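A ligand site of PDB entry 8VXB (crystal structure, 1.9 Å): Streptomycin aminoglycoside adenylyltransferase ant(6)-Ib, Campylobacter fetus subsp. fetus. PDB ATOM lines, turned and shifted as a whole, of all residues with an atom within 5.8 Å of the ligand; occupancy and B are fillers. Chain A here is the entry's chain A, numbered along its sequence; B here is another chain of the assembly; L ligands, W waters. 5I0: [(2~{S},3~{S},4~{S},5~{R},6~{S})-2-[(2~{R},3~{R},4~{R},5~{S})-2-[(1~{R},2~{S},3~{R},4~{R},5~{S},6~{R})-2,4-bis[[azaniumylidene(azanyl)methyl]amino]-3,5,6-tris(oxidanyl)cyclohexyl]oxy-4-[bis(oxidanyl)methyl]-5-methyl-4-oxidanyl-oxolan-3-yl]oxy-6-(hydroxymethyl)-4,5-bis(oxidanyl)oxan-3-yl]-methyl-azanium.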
ATOM      1  N   GLU A  29      22.288  -3.124 -13.230  1.00  0.00           N
ATOM      2  CA  GLU A  29      22.865  -3.854 -12.113  1.00  0.00           C
ATOM      3  C   GLU A  29      22.303  -5.262 -12.140  1.00  0.00           C
ATOM      4  O   GLU A  29      21.339  -5.548 -12.846  1.00  0.00           O
ATOM      5  CB  GLU A  29      22.524  -3.191 -10.751  1.00  0.00           C
ATOM      6  CG  GLU A  29      23.269  -1.890 -10.477  1.00  0.00           C
ATOM      7  CD  GLU A  29      22.739  -1.119  -9.260  1.00  0.00           C
ATOM      8  OE1 GLU A  29      23.350  -0.070  -8.902  1.00  0.00           O
ATOM      9  OE2 GLU A  29      21.776  -1.609  -8.604  1.00  0.00           O
ATOM     10  N   GLY A  30      22.887  -6.159 -11.347  1.00  0.00           N
ATOM     11  CA  GLY A  30      22.198  -7.427 -11.090  1.00  0.00           C
ATOM     12  C   GLY A  30      22.440  -8.474 -12.154  1.00  0.00           C
ATOM     13  O   GLY A  30      23.394  -8.417 -12.944  1.00  0.00           O
ATOM     14  N   ASP A  44      14.864  -9.476 -13.067  1.00  0.00           N
ATOM     15  CA  ASP A  44      14.450  -8.093 -12.904  1.00  0.00           C
ATOM     16  C   ASP A  44      15.302  -7.192 -13.797  1.00  0.00           C
ATOM     17  O   ASP A  44      16.425  -7.554 -14.174  1.00  0.00           O
ATOM     18  CB  ASP A  44      14.623  -7.633 -11.436  1.00  0.00           C
ATOM     19  CG  ASP A  44      13.836  -8.503 -10.442  1.00  0.00           C
ATOM     20  OD1 ASP A  44      12.896  -9.223 -10.850  1.00  0.00           O
ATOM     21  OD2 ASP A  44      14.123  -8.398  -9.217  1.00  0.00           O
ATOM     22  N   ASP A  46      17.241  -4.124 -13.116  1.00  0.00           N
ATOM     23  CA  ASP A  46      17.772  -3.287 -12.030  1.00  0.00           C
ATOM     24  C   ASP A  46      18.491  -2.098 -12.651  1.00  0.00           C
ATOM     25  O   ASP A  46      19.612  -2.220 -13.129  1.00  0.00           O
ATOM     26  CB  ASP A  46      18.712  -4.067 -11.115  1.00  0.00           C
ATOM     27  CG  ASP A  46      18.032  -5.264 -10.422  1.00  0.00           C
ATOM     28  OD1 ASP A  46      16.806  -5.171 -10.128  1.00  0.00           O
ATOM     29  OD2 ASP A  46      18.697  -6.293 -10.176  1.00  0.00           O
ATOM     30  N   ILE A  47      17.833  -0.939 -12.640  1.00  0.00           N
ATOM     31  CA  ILE A  47      18.272   0.245 -13.375  1.00  0.00           C
ATOM     32  C   ILE A  47      18.551   1.351 -12.364  1.00  0.00           C
ATOM     33  O   ILE A  47      17.753   1.565 -11.438  1.00  0.00           O
ATOM     34  CB  ILE A  47      17.184   0.710 -14.376  1.00  0.00           C
ATOM     35  CG1 ILE A  47      16.832  -0.376 -15.399  1.00  0.00           C
ATOM     36  CG2 ILE A  47      17.613   2.022 -15.110  1.00  0.00           C
ATOM     37  CD1 ILE A  47      17.907  -0.653 -16.422  1.00  0.00           C
ATOM     38  N   THR A  48      19.628   2.081 -12.560  1.00  0.00           N
ATOM     39  CA  THR A  48      19.970   3.213 -11.706  1.00  0.00           C
ATOM     40  C   THR A  48      20.104   4.457 -12.572  1.00  0.00           C
ATOM     41  O   THR A  48      20.790   4.433 -13.593  1.00  0.00           O
ATOM     42  CB  THR A  48      21.263   2.920 -10.918  1.00  0.00           C
ATOM     43  OG1 THR A  48      21.025   1.827 -10.016  1.00  0.00           O
ATOM     44  CG2 THR A  48      21.660   4.123 -10.095  1.00  0.00           C
ATOM     45  N   GLN A  74       6.625  -0.831  -4.514  1.00  0.00           N
ATOM     46  CA  GLN A  74       7.130  -0.417  -3.208  1.00  0.00           C
ATOM     47  C   GLN A  74       8.101   0.729  -3.393  1.00  0.00           C
ATOM     48  O   GLN A  74       8.870   0.735  -4.360  1.00  0.00           O
ATOM     49  CB  GLN A  74       7.857  -1.588  -2.496  1.00  0.00           C
ATOM     50  CG  GLN A  74       8.242  -1.264  -1.039  1.00  0.00           C
ATOM     51  CD  GLN A  74       8.860  -2.477  -0.333  1.00  0.00           C
ATOM     52  OE1 GLN A  74      10.084  -2.528  -0.120  1.00  0.00           O
ATOM     53  NE2 GLN A  74       8.023  -3.428   0.098  1.00  0.00           N
ATOM     54  N   PRO A  76      10.849   1.810  -1.055  1.00  0.00           N
ATOM     55  CA  PRO A  76      11.385   1.351   0.237  1.00  0.00           C
ATOM     56  C   PRO A  76      12.147   2.414   0.996  1.00  0.00           C
ATOM     57  O   PRO A  76      12.371   2.248   2.197  1.00  0.00           O
ATOM     58  CB  PRO A  76      12.306   0.179  -0.125  1.00  0.00           C
ATOM     59  CG  PRO A  76      12.384   0.097  -1.579  1.00  0.00           C
ATOM     60  CD  PRO A  76      11.466   1.136  -2.208  1.00  0.00           C
ATOM     61  N   GLU A  77      12.580   3.478   0.343  1.00  0.00           N
ATOM     62  CA  GLU A  77      13.233   4.565   1.081  1.00  0.00           C
ATOM     63  C   GLU A  77      12.231   5.631   1.502  1.00  0.00           C
ATOM     64  O   GLU A  77      12.633   6.715   1.931  1.00  0.00           O
ATOM     65  CB  GLU A  77      14.372   5.141   0.237  1.00  0.00           C
ATOM     66  CG  GLU A  77      15.602   4.189   0.181  1.00  0.00           C
ATOM     67  CD  GLU A  77      15.396   3.007  -0.760  1.00  0.00           C
ATOM     68  OE1 GLU A  77      15.028   3.231  -1.927  1.00  0.00           O
ATOM     69  OE2 GLU A  77      15.601   1.832  -0.348  1.00  0.00           O
ATOM     70  N   MET A  79       9.110   4.662   3.403  1.00  0.00           N
ATOM     71  CA  MET A  79       8.084   4.045   4.227  1.00  0.00           C
ATOM     72  C   MET A  79       8.247   4.433   5.682  1.00  0.00           C
ATOM     73  O   MET A  79       9.278   4.951   6.106  1.00  0.00           O
ATOM     74  CB  MET A  79       8.032   2.505   4.113  1.00  0.00           C
ATOM     75  CG  MET A  79       7.871   1.927   2.712  1.00  0.00           C
ATOM     76  SD  MET A  79       8.536   0.275   2.449  1.00  0.00           S
ATOM     77  CE  MET A  79       6.964  -0.607   2.486  1.00  0.00           C
ATOM     78  N   PHE A  82       9.588   0.805   7.842  1.00  0.00           N
ATOM     79  CA  PHE A  82      10.904   0.309   7.525  1.00  0.00           C
ATOM     80  C   PHE A  82      11.874   1.476   7.311  1.00  0.00           C
ATOM     81  O   PHE A  82      11.569   2.395   6.545  1.00  0.00           O
ATOM     82  CB  PHE A  82      10.836  -0.555   6.240  1.00  0.00           C
ATOM     83  CG  PHE A  82       9.909  -1.761   6.358  1.00  0.00           C
ATOM     84  CD1 PHE A  82      10.326  -2.904   7.003  1.00  0.00           C
ATOM     85  CD2 PHE A  82       8.649  -1.733   5.788  1.00  0.00           C
ATOM     86  CE1 PHE A  82       9.494  -4.029   7.099  1.00  0.00           C
ATOM     87  CE2 PHE A  82       7.810  -2.856   5.868  1.00  0.00           C
ATOM     88  CZ  PHE A  82       8.242  -3.995   6.532  1.00  0.00           C
ATOM     89  N   PRO A  83      13.027   1.475   7.966  1.00  0.00           N
ATOM     90  CA  PRO A  83      13.997   2.561   7.758  1.00  0.00           C
ATOM     91  C   PRO A  83      14.729   2.397   6.430  1.00  0.00           C
ATOM     92  O   PRO A  83      14.717   1.329   5.811  1.00  0.00           O
ATOM     93  CB  PRO A  83      14.960   2.408   8.948  1.00  0.00           C
ATOM     94  CG  PRO A  83      14.980   0.925   9.203  1.00  0.00           C
ATOM     95  CD  PRO A  83      13.520   0.459   8.921  1.00  0.00           C
ATOM     96  N   GLU A  85      17.641   1.619   4.063  1.00  0.00           N
ATOM     97  CA  GLU A  85      18.814   0.756   4.119  1.00  0.00           C
ATOM     98  C   GLU A  85      19.629   0.784   2.833  1.00  0.00           C
ATOM     99  O   GLU A  85      20.617   0.063   2.739  1.00  0.00           O
ATOM    100  CB  GLU A  85      18.396  -0.691   4.443  1.00  0.00           C
ATOM    101  CG  GLU A  85      17.539  -0.775   5.706  1.00  0.00           C
ATOM    102  CD  GLU A  85      17.445  -2.201   6.259  1.00  0.00           C
ATOM    103  OE1 GLU A  85      17.821  -3.152   5.534  1.00  0.00           O
ATOM    104  OE2 GLU A  85      17.024  -2.358   7.426  1.00  0.00           O
ATOM    105  N   GLU A  86      19.217   1.554   1.838  1.00  0.00           N
ATOM    106  CA  GLU A  86      19.977   1.786   0.627  1.00  0.00           C
ATOM    107  C   GLU A  86      20.123   3.283   0.441  1.00  0.00           C
ATOM    108  O   GLU A  86      19.313   4.061   0.954  1.00  0.00           O
ATOM    109  CB  GLU A  86      19.315   1.192  -0.625  1.00  0.00           C
ATOM    110  CG  GLU A  86      18.846  -0.274  -0.538  1.00  0.00           C
ATOM    111  CD  GLU A  86      19.994  -1.278  -0.501  1.00  0.00           C
ATOM    112  OE1 GLU A  86      21.133  -0.955  -0.948  1.00  0.00           O
ATOM    113  OE2 GLU A  86      19.738  -2.427  -0.067  1.00  0.00           O
ATOM    114  N   SER A  90      14.319   4.529  -4.373  1.00  0.00           N
ATOM    115  CA  SER A  90      14.028   3.494  -5.349  1.00  0.00           C
ATOM    116  C   SER A  90      12.525   3.189  -5.457  1.00  0.00           C
ATOM    117  O   SER A  90      11.718   3.528  -4.587  1.00  0.00           O
ATOM    118  CB  SER A  90      14.800   2.200  -5.054  1.00  0.00           C
ATOM    119  OG  SER A  90      14.469   1.691  -3.781  1.00  0.00           O
ATOM    120  N   LEU A  92      10.320  -0.202  -6.621  1.00  0.00           N
ATOM    121  CA  LEU A  92      10.313  -1.619  -6.972  1.00  0.00           C
ATOM    122  C   LEU A  92       8.946  -1.901  -7.581  1.00  0.00           C
ATOM    123  O   LEU A  92       7.941  -1.851  -6.868  1.00  0.00           O
ATOM    124  CB  LEU A  92      10.565  -2.492  -5.740  1.00  0.00           C
ATOM    125  CG  LEU A  92      11.707  -1.997  -4.825  1.00  0.00           C
ATOM    126  CD1 LEU A  92      11.883  -3.029  -3.673  1.00  0.00           C
ATOM    127  CD2 LEU A  92      12.978  -1.869  -5.600  1.00  0.00           C
ATOM    128  N   ASP A 102      13.303  -2.579 -10.994  1.00  0.00           N
ATOM    129  CA  ASP A 102      13.721  -1.980  -9.720  1.00  0.00           C
ATOM    130  C   ASP A 102      14.563  -0.771 -10.122  1.00  0.00           C
ATOM    131  O   ASP A 102      15.698  -0.933 -10.571  1.00  0.00           O
ATOM    132  CB  ASP A 102      14.506  -2.968  -8.861  1.00  0.00           C
ATOM    133  CG  ASP A 102      13.622  -4.153  -8.370  1.00  0.00           C
ATOM    134  OD1 ASP A 102      12.379  -4.126  -8.589  1.00  0.00           O
ATOM    135  OD2 ASP A 102      14.174  -5.100  -7.749  1.00  0.00           O
ATOM    136  N   THR A 104      16.407   2.776  -9.283  1.00  0.00           N
ATOM    137  CA  THR A 104      17.061   3.568  -8.233  1.00  0.00           C
ATOM    138  C   THR A 104      17.454   4.938  -8.766  1.00  0.00           C
ATOM    139  O   THR A 104      18.066   5.044  -9.823  1.00  0.00           O
ATOM    140  CB  THR A 104      18.318   2.861  -7.693  1.00  0.00           C
ATOM    141  OG1 THR A 104      17.964   1.551  -7.198  1.00  0.00           O
ATOM    142  CG2 THR A 104      18.966   3.675  -6.545  1.00  0.00           C
ATOM    143  N   ASN B 157       2.288  -4.232   2.133  1.00  0.00           N
ATOM    144  CA  ASN B 157       3.093  -4.056   0.937  1.00  0.00           C
ATOM    145  C   ASN B 157       4.302  -4.991   0.960  1.00  0.00           C
ATOM    146  O   ASN B 157       4.566  -5.699  -0.002  1.00  0.00           O
ATOM    147  CB  ASN B 157       3.523  -2.573   0.825  1.00  0.00           C
ATOM    148  CG  ASN B 157       4.186  -2.274  -0.504  1.00  0.00           C
ATOM    149  OD1 ASN B 157       5.315  -2.704  -0.756  1.00  0.00           O
ATOM    150  ND2 ASN B 157       3.495  -1.541  -1.358  1.00  0.00           N
ATOM    151  N   GLU B 158       5.032  -5.020   2.081  1.00  0.00           N
ATOM    152  CA  GLU B 158       6.218  -5.885   2.169  1.00  0.00           C
ATOM    153  C   GLU B 158       5.842  -7.356   2.134  1.00  0.00           C
ATOM    154  O   GLU B 158       6.514  -8.160   1.477  1.00  0.00           O
ATOM    155  CB  GLU B 158       7.035  -5.571   3.442  1.00  0.00           C
ATOM    156  CG  GLU B 158       8.344  -6.406   3.524  1.00  0.00           C
ATOM    157  CD  GLU B 158       9.442  -5.996   2.528  1.00  0.00           C
ATOM    158  OE1 GLU B 158       9.131  -5.663   1.358  1.00  0.00           O
ATOM    159  OE2 GLU B 158      10.652  -6.140   2.859  1.00  0.00           O
ATOM    160  N   ASN B 161       4.611  -8.005  -1.703  1.00  0.00           N
ATOM    161  CA  ASN B 161       5.752  -7.898  -2.619  1.00  0.00           C
ATOM    162  C   ASN B 161       6.737  -9.048  -2.479  1.00  0.00           C
ATOM    163  O   ASN B 161       7.175  -9.626  -3.486  1.00  0.00           O
ATOM    164  CB  ASN B 161       6.472  -6.564  -2.425  1.00  0.00           C
ATOM    165  CG  ASN B 161       7.209  -6.157  -3.676  1.00  0.00           C
ATOM    166  OD1 ASN B 161       6.619  -6.092  -4.760  1.00  0.00           O
ATOM    167  ND2 ASN B 161       8.479  -5.752  -3.513  1.00  0.00           N
ATOM    168  N   THR B 162       7.067  -9.435  -1.239  1.00  0.00           N
ATOM    169  CA  THR B 162       8.065 -10.484  -1.078  1.00  0.00           C
ATOM    170  C   THR B 162       7.515 -11.867  -1.410  1.00  0.00           C
ATOM    171  O   THR B 162       8.274 -12.753  -1.846  1.00  0.00           O
ATOM    172  CB  THR B 162       8.659 -10.407   0.341  1.00  0.00           C
ATOM    173  OG1 THR B 162       8.997  -9.039   0.624  1.00  0.00           O
ATOM    174  CG2 THR B 162       9.949 -11.266   0.417  1.00  0.00           C
ATOM    175  N   TYR B 165       8.862 -12.962  -4.588  1.00  0.00           N
ATOM    176  CA  TYR B 165      10.208 -13.531  -4.590  1.00  0.00           C
ATOM    177  C   TYR B 165      10.210 -15.017  -4.227  1.00  0.00           C
ATOM    178  O   TYR B 165      11.090 -15.761  -4.661  1.00  0.00           O
ATOM    179  CB  TYR B 165      11.107 -12.791  -3.611  1.00  0.00           C
ATOM    180  CG  TYR B 165      11.563 -11.429  -4.070  1.00  0.00           C
ATOM    181  CD1 TYR B 165      10.674 -10.371  -4.169  1.00  0.00           C
ATOM    182  CD2 TYR B 165      12.905 -11.193  -4.346  1.00  0.00           C
ATOM    183  CE1 TYR B 165      11.105  -9.086  -4.567  1.00  0.00           C
ATOM    184  CE2 TYR B 165      13.353  -9.928  -4.752  1.00  0.00           C
ATOM    185  CZ  TYR B 165      12.441  -8.886  -4.862  1.00  0.00           C
ATOM    186  OH  TYR B 165      12.892  -7.637  -5.252  1.00  0.00           O
ATOM    187  N   HIS B 181      13.584 -16.290   1.635  1.00  0.00           N
ATOM    188  CA  HIS B 181      12.690 -15.140   1.582  1.00  0.00           C
ATOM    189  C   HIS B 181      11.418 -15.377   2.381  1.00  0.00           C
ATOM    190  O   HIS B 181      10.871 -14.436   2.951  1.00  0.00           O
ATOM    191  CB  HIS B 181      12.372 -14.783   0.121  1.00  0.00           C
ATOM    192  CG  HIS B 181      13.514 -14.074  -0.551  1.00  0.00           C
ATOM    193  ND1 HIS B 181      14.613 -14.758  -1.023  1.00  0.00           N
ATOM    194  CD2 HIS B 181      13.775 -12.764  -0.711  1.00  0.00           C
ATOM    195  CE1 HIS B 181      15.497 -13.882  -1.504  1.00  0.00           C
ATOM    196  NE2 HIS B 181      15.010 -12.669  -1.323  1.00  0.00           N
ATOM    197  N   ILE B 185      11.459 -12.869   5.650  1.00  0.00           N
ATOM    198  CA  ILE B 185      10.638 -11.700   5.366  1.00  0.00           C
ATOM    199  C   ILE B 185       9.158 -12.020   5.381  1.00  0.00           C
ATOM    200  O   ILE B 185       8.415 -11.424   6.173  1.00  0.00           O
ATOM    201  CB  ILE B 185      11.023 -11.055   4.024  1.00  0.00           C
ATOM    202  CG1 ILE B 185      12.472 -10.547   4.056  1.00  0.00           C
ATOM    203  CG2 ILE B 185      10.086  -9.890   3.721  1.00  0.00           C
ATOM    204  CD1 ILE B 185      13.039 -10.334   2.668  1.00  0.00           C
HETATM  205  C11 5I0 L   1      17.835  -4.465  -5.315  1.00  0.00           C
HETATM  206  C12 5I0 L   1      14.551  -5.549  -1.273  1.00  0.00           C
HETATM  207  C13 5I0 L   1      13.359  -3.397   0.834  1.00  0.00           C
HETATM  208  NB1 5I0 L   1      20.603  -3.945  -7.628  1.00  0.00           N
HETATM  209  CG2 5I0 L   1      11.015  -6.496  -1.450  1.00  0.00           C
HETATM  210  CD1 5I0 L   1      15.942  -1.557  -2.228  1.00  0.00           C
HETATM  211  NE1 5I0 L   1      15.571  -0.985  -1.098  1.00  0.00           N
HETATM  212  CH2 5I0 L   1      13.329  -8.944  -1.233  1.00  0.00           C
HETATM  213  C21 5I0 L   1      17.811  -3.626  -4.044  1.00  0.00           C
HETATM  214  C22 5I0 L   1      13.148  -5.253  -0.738  1.00  0.00           C
HETATM  215  C23 5I0 L   1      12.731  -3.087   2.167  1.00  0.00           C
HETATM  216  C31 5I0 L   1      16.429  -3.648  -3.415  1.00  0.00           C
HETATM  217  C32 5I0 L   1      12.396  -6.622  -0.801  1.00  0.00           C
HETATM  218  C33 5I0 L   1      13.520  -3.753   3.286  1.00  0.00           C
HETATM  219  C41 5I0 L   1      16.001  -5.085  -3.111  1.00  0.00           C
HETATM  220  C42 5I0 L   1      13.361  -7.505  -1.601  1.00  0.00           C
HETATM  221  C43 5I0 L   1      14.999  -3.400   3.193  1.00  0.00           C
HETATM  222  C51 5I0 L   1      15.989  -5.900  -4.397  1.00  0.00           C
HETATM  223  C53 5I0 L   1      15.519  -3.735   1.792  1.00  0.00           C
HETATM  224  C61 5I0 L   1      17.377  -5.895  -5.042  1.00  0.00           C
HETATM  225  C63 5I0 L   1      16.950  -3.314   1.586  1.00  0.00           C
HETATM  226  CA1 5I0 L   1      19.488  -3.704  -6.961  1.00  0.00           C
HETATM  227  CI3 5I0 L   1      10.488  -2.690   3.040  1.00  0.00           C
HETATM  228  N11 5I0 L   1      19.157  -4.446  -5.919  1.00  0.00           N
HETATM  229  N23 5I0 L   1      11.321  -3.494   2.182  1.00  0.00           N
HETATM  230  N31 5I0 L   1      16.367  -2.816  -2.223  1.00  0.00           N
HETATM  231  NC1 5I0 L   1      18.712  -2.708  -7.346  1.00  0.00           N
HETATM  232  NF1 5I0 L   1      15.890  -0.885  -3.370  1.00  0.00           N
HETATM  233  O13 5I0 L   1      13.205  -4.788   0.604  1.00  0.00           O
HETATM  234  O21 5I0 L   1      18.211  -2.283  -4.343  1.00  0.00           O
HETATM  235  O32 5I0 L   1      12.223  -7.176   0.502  1.00  0.00           O
HETATM  236  O33 5I0 L   1      13.011  -3.392   4.559  1.00  0.00           O
HETATM  237  O41 5I0 L   1      14.678  -5.033  -2.559  1.00  0.00           O
HETATM  238  O42 5I0 L   1      14.640  -6.962  -1.287  1.00  0.00           O
HETATM  239  O43 5I0 L   1      15.724  -4.183   4.137  1.00  0.00           O
HETATM  240  O51 5I0 L   1      15.575  -7.240  -4.130  1.00  0.00           O
HETATM  241  O53 5I0 L   1      14.725  -3.037   0.815  1.00  0.00           O
HETATM  242  O61 5I0 L   1      17.429  -6.657  -6.232  1.00  0.00           O
HETATM  243  O63 5I0 L   1      17.399  -3.623   0.279  1.00  0.00           O
HETATM  244 OG2A 5I0 L   1      10.425  -7.785  -1.601  1.00  0.00           O
HETATM  245 OG2B 5I0 L   1      10.388  -5.309  -0.991  1.00  0.00           O
HETATM  246  O   HOH W   1      13.464   0.109   3.369  1.00  0.00           O
HETATM  247  O   HOH W   2      18.540   0.932  -4.495  1.00  0.00           O
HETATM  248  O   HOH W   3      13.297  -4.969   6.787  1.00  0.00           O
HETATM  249  O   HOH W   4      17.169  -8.622  -2.600  1.00  0.00           O
HETATM  250  O   HOH W   5      11.834  -6.637   5.062  1.00  0.00           O
HETATM  251  O   HOH W   6      14.445  -7.169   4.501  1.00  0.00           O
HETATM  252  O   HOH W   7      14.289  -1.381   6.325  1.00  0.00           O
HETATM  253  O   HOH W   8      18.394  -0.328  -9.182  1.00  0.00           O
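OE2 of Glu 86 lies within hydrogen-bond range of O63 of the ligand (2.6 Å).
N23 of the ligand is in salt-bridge range of OE2 of Glu 158 of chain B (2.8 Å).
The side-chain carboxylate (OE1) of Glu 85 sits at hydrogen-bond distance from an oxygen (O43) of the ligand, 2.7 Å away.
OE1 of Gln 74 sits at hydrogen-bond distance from N23 of the ligand (2.8 Å).
OE2 of Glu 29 is in salt-bridge range of NB1 of the ligand (2.8 Å).
The side-chain carboxylate of Glu 77 is in salt-bridge range of a nitrogen (NE1) of the ligand.
OG2A of the ligand is in hydrogen-bond range of OG1 of Thr 162 of chain B (2.9 Å).
An oxygen (O51) of the ligand lies within hydrogen-bond range of the side-chain hydroxyl of Tyr 165 of chain B, at 2.9 Å.
NF1 of the ligand lies within hydrogen-bond range of OG of Ser 90, at 3.0 Å.
An oxygen (OG2B) of the ligand sits at hydrogen-bond distance from the side-chain amide nitrogen (ND2) of Asn 161 of chain B, 3.2 Å away.
A nitrogen (NB1) of the ligand lies within salt-bridge range of the side-chain carboxylate (OD2) of Asp 46 (3.95 Å).
The side-chain amide nitrogen of Gln 74 is in hydrogen-bond range of the side-chain carboxylate of Glu 158 of chain B (2.8 Å).
OG1 of Thr 162 of chain B lies within hydrogen-bond range of O of Glu 158 of chain B.
The backbone NH (N) of Leu 92 sits at hydrogen-bond distance from the backbone carbonyl oxygen (O) of Gln 74 (2.8 Å).
NE2 of Gln 74 lies within hydrogen-bond range of OD1 of Asn 157 of chain B.
N of Glu 29 is in hydrogen-bond range of O of Asp 46 (2.8 Å).
The side-chain carboxylate of Glu 29 sits at hydrogen-bond distance from the side-chain hydroxyl of Thr 48, at 3.2 Å.
OG of Ser 90 sits at hydrogen-bond distance from OE1 of Glu 77 (2.5 Å).
The backbone carbonyl oxygen (O) of Asp 102 is in hydrogen-bond range of the backbone NH (N) of Ile 47 (3.0 Å).
Merely in contact with the ligand: Pro 76, Met 79, Phe 82, Leu 92, Asp 102, His 181 of chain B and Ile 185 of chain B.
Hydrophobic or aromatic side chains that line the ligand: Pro 76, Met 79, Phe 82, Leu 92, Tyr 165 of chain B, His 181 of chain B and Ile 185 of chain B.
Along chain A the residues within 4 Å of the ligand span positions 29 to 102.
Water W7 lies within hydrogen-bond range of O of Pro 83 (2.8 Å), O33 of the ligand (3.0 Å) and OE2 of Glu 85 (3.1 Å).
Water W8 lies within hydrogen-bond range of the side-chain hydroxyl of Thr 104 (2.8 Å), the backbone carbonyl oxygen of Ile 47 (3.0 Å), a nitrogen (NC1) of the ligand (3.0 Å) and the backbone carbonyl oxygen of Asp 102 (3.1 Å).
Water W2 bridges OG1 of Thr 104 (2.8 Å) and O21 of the ligand (3.2 Å).
Water W5 bridges the side-chain carboxylate of Glu 158 of chain B (2.5 Å) and an oxygen (O33) of the ligand (3.5 Å).
Water W1 lies within hydrogen-bond range of O of Pro 76 (2.7 Å) and O of Pro 83 (3.0 Å).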
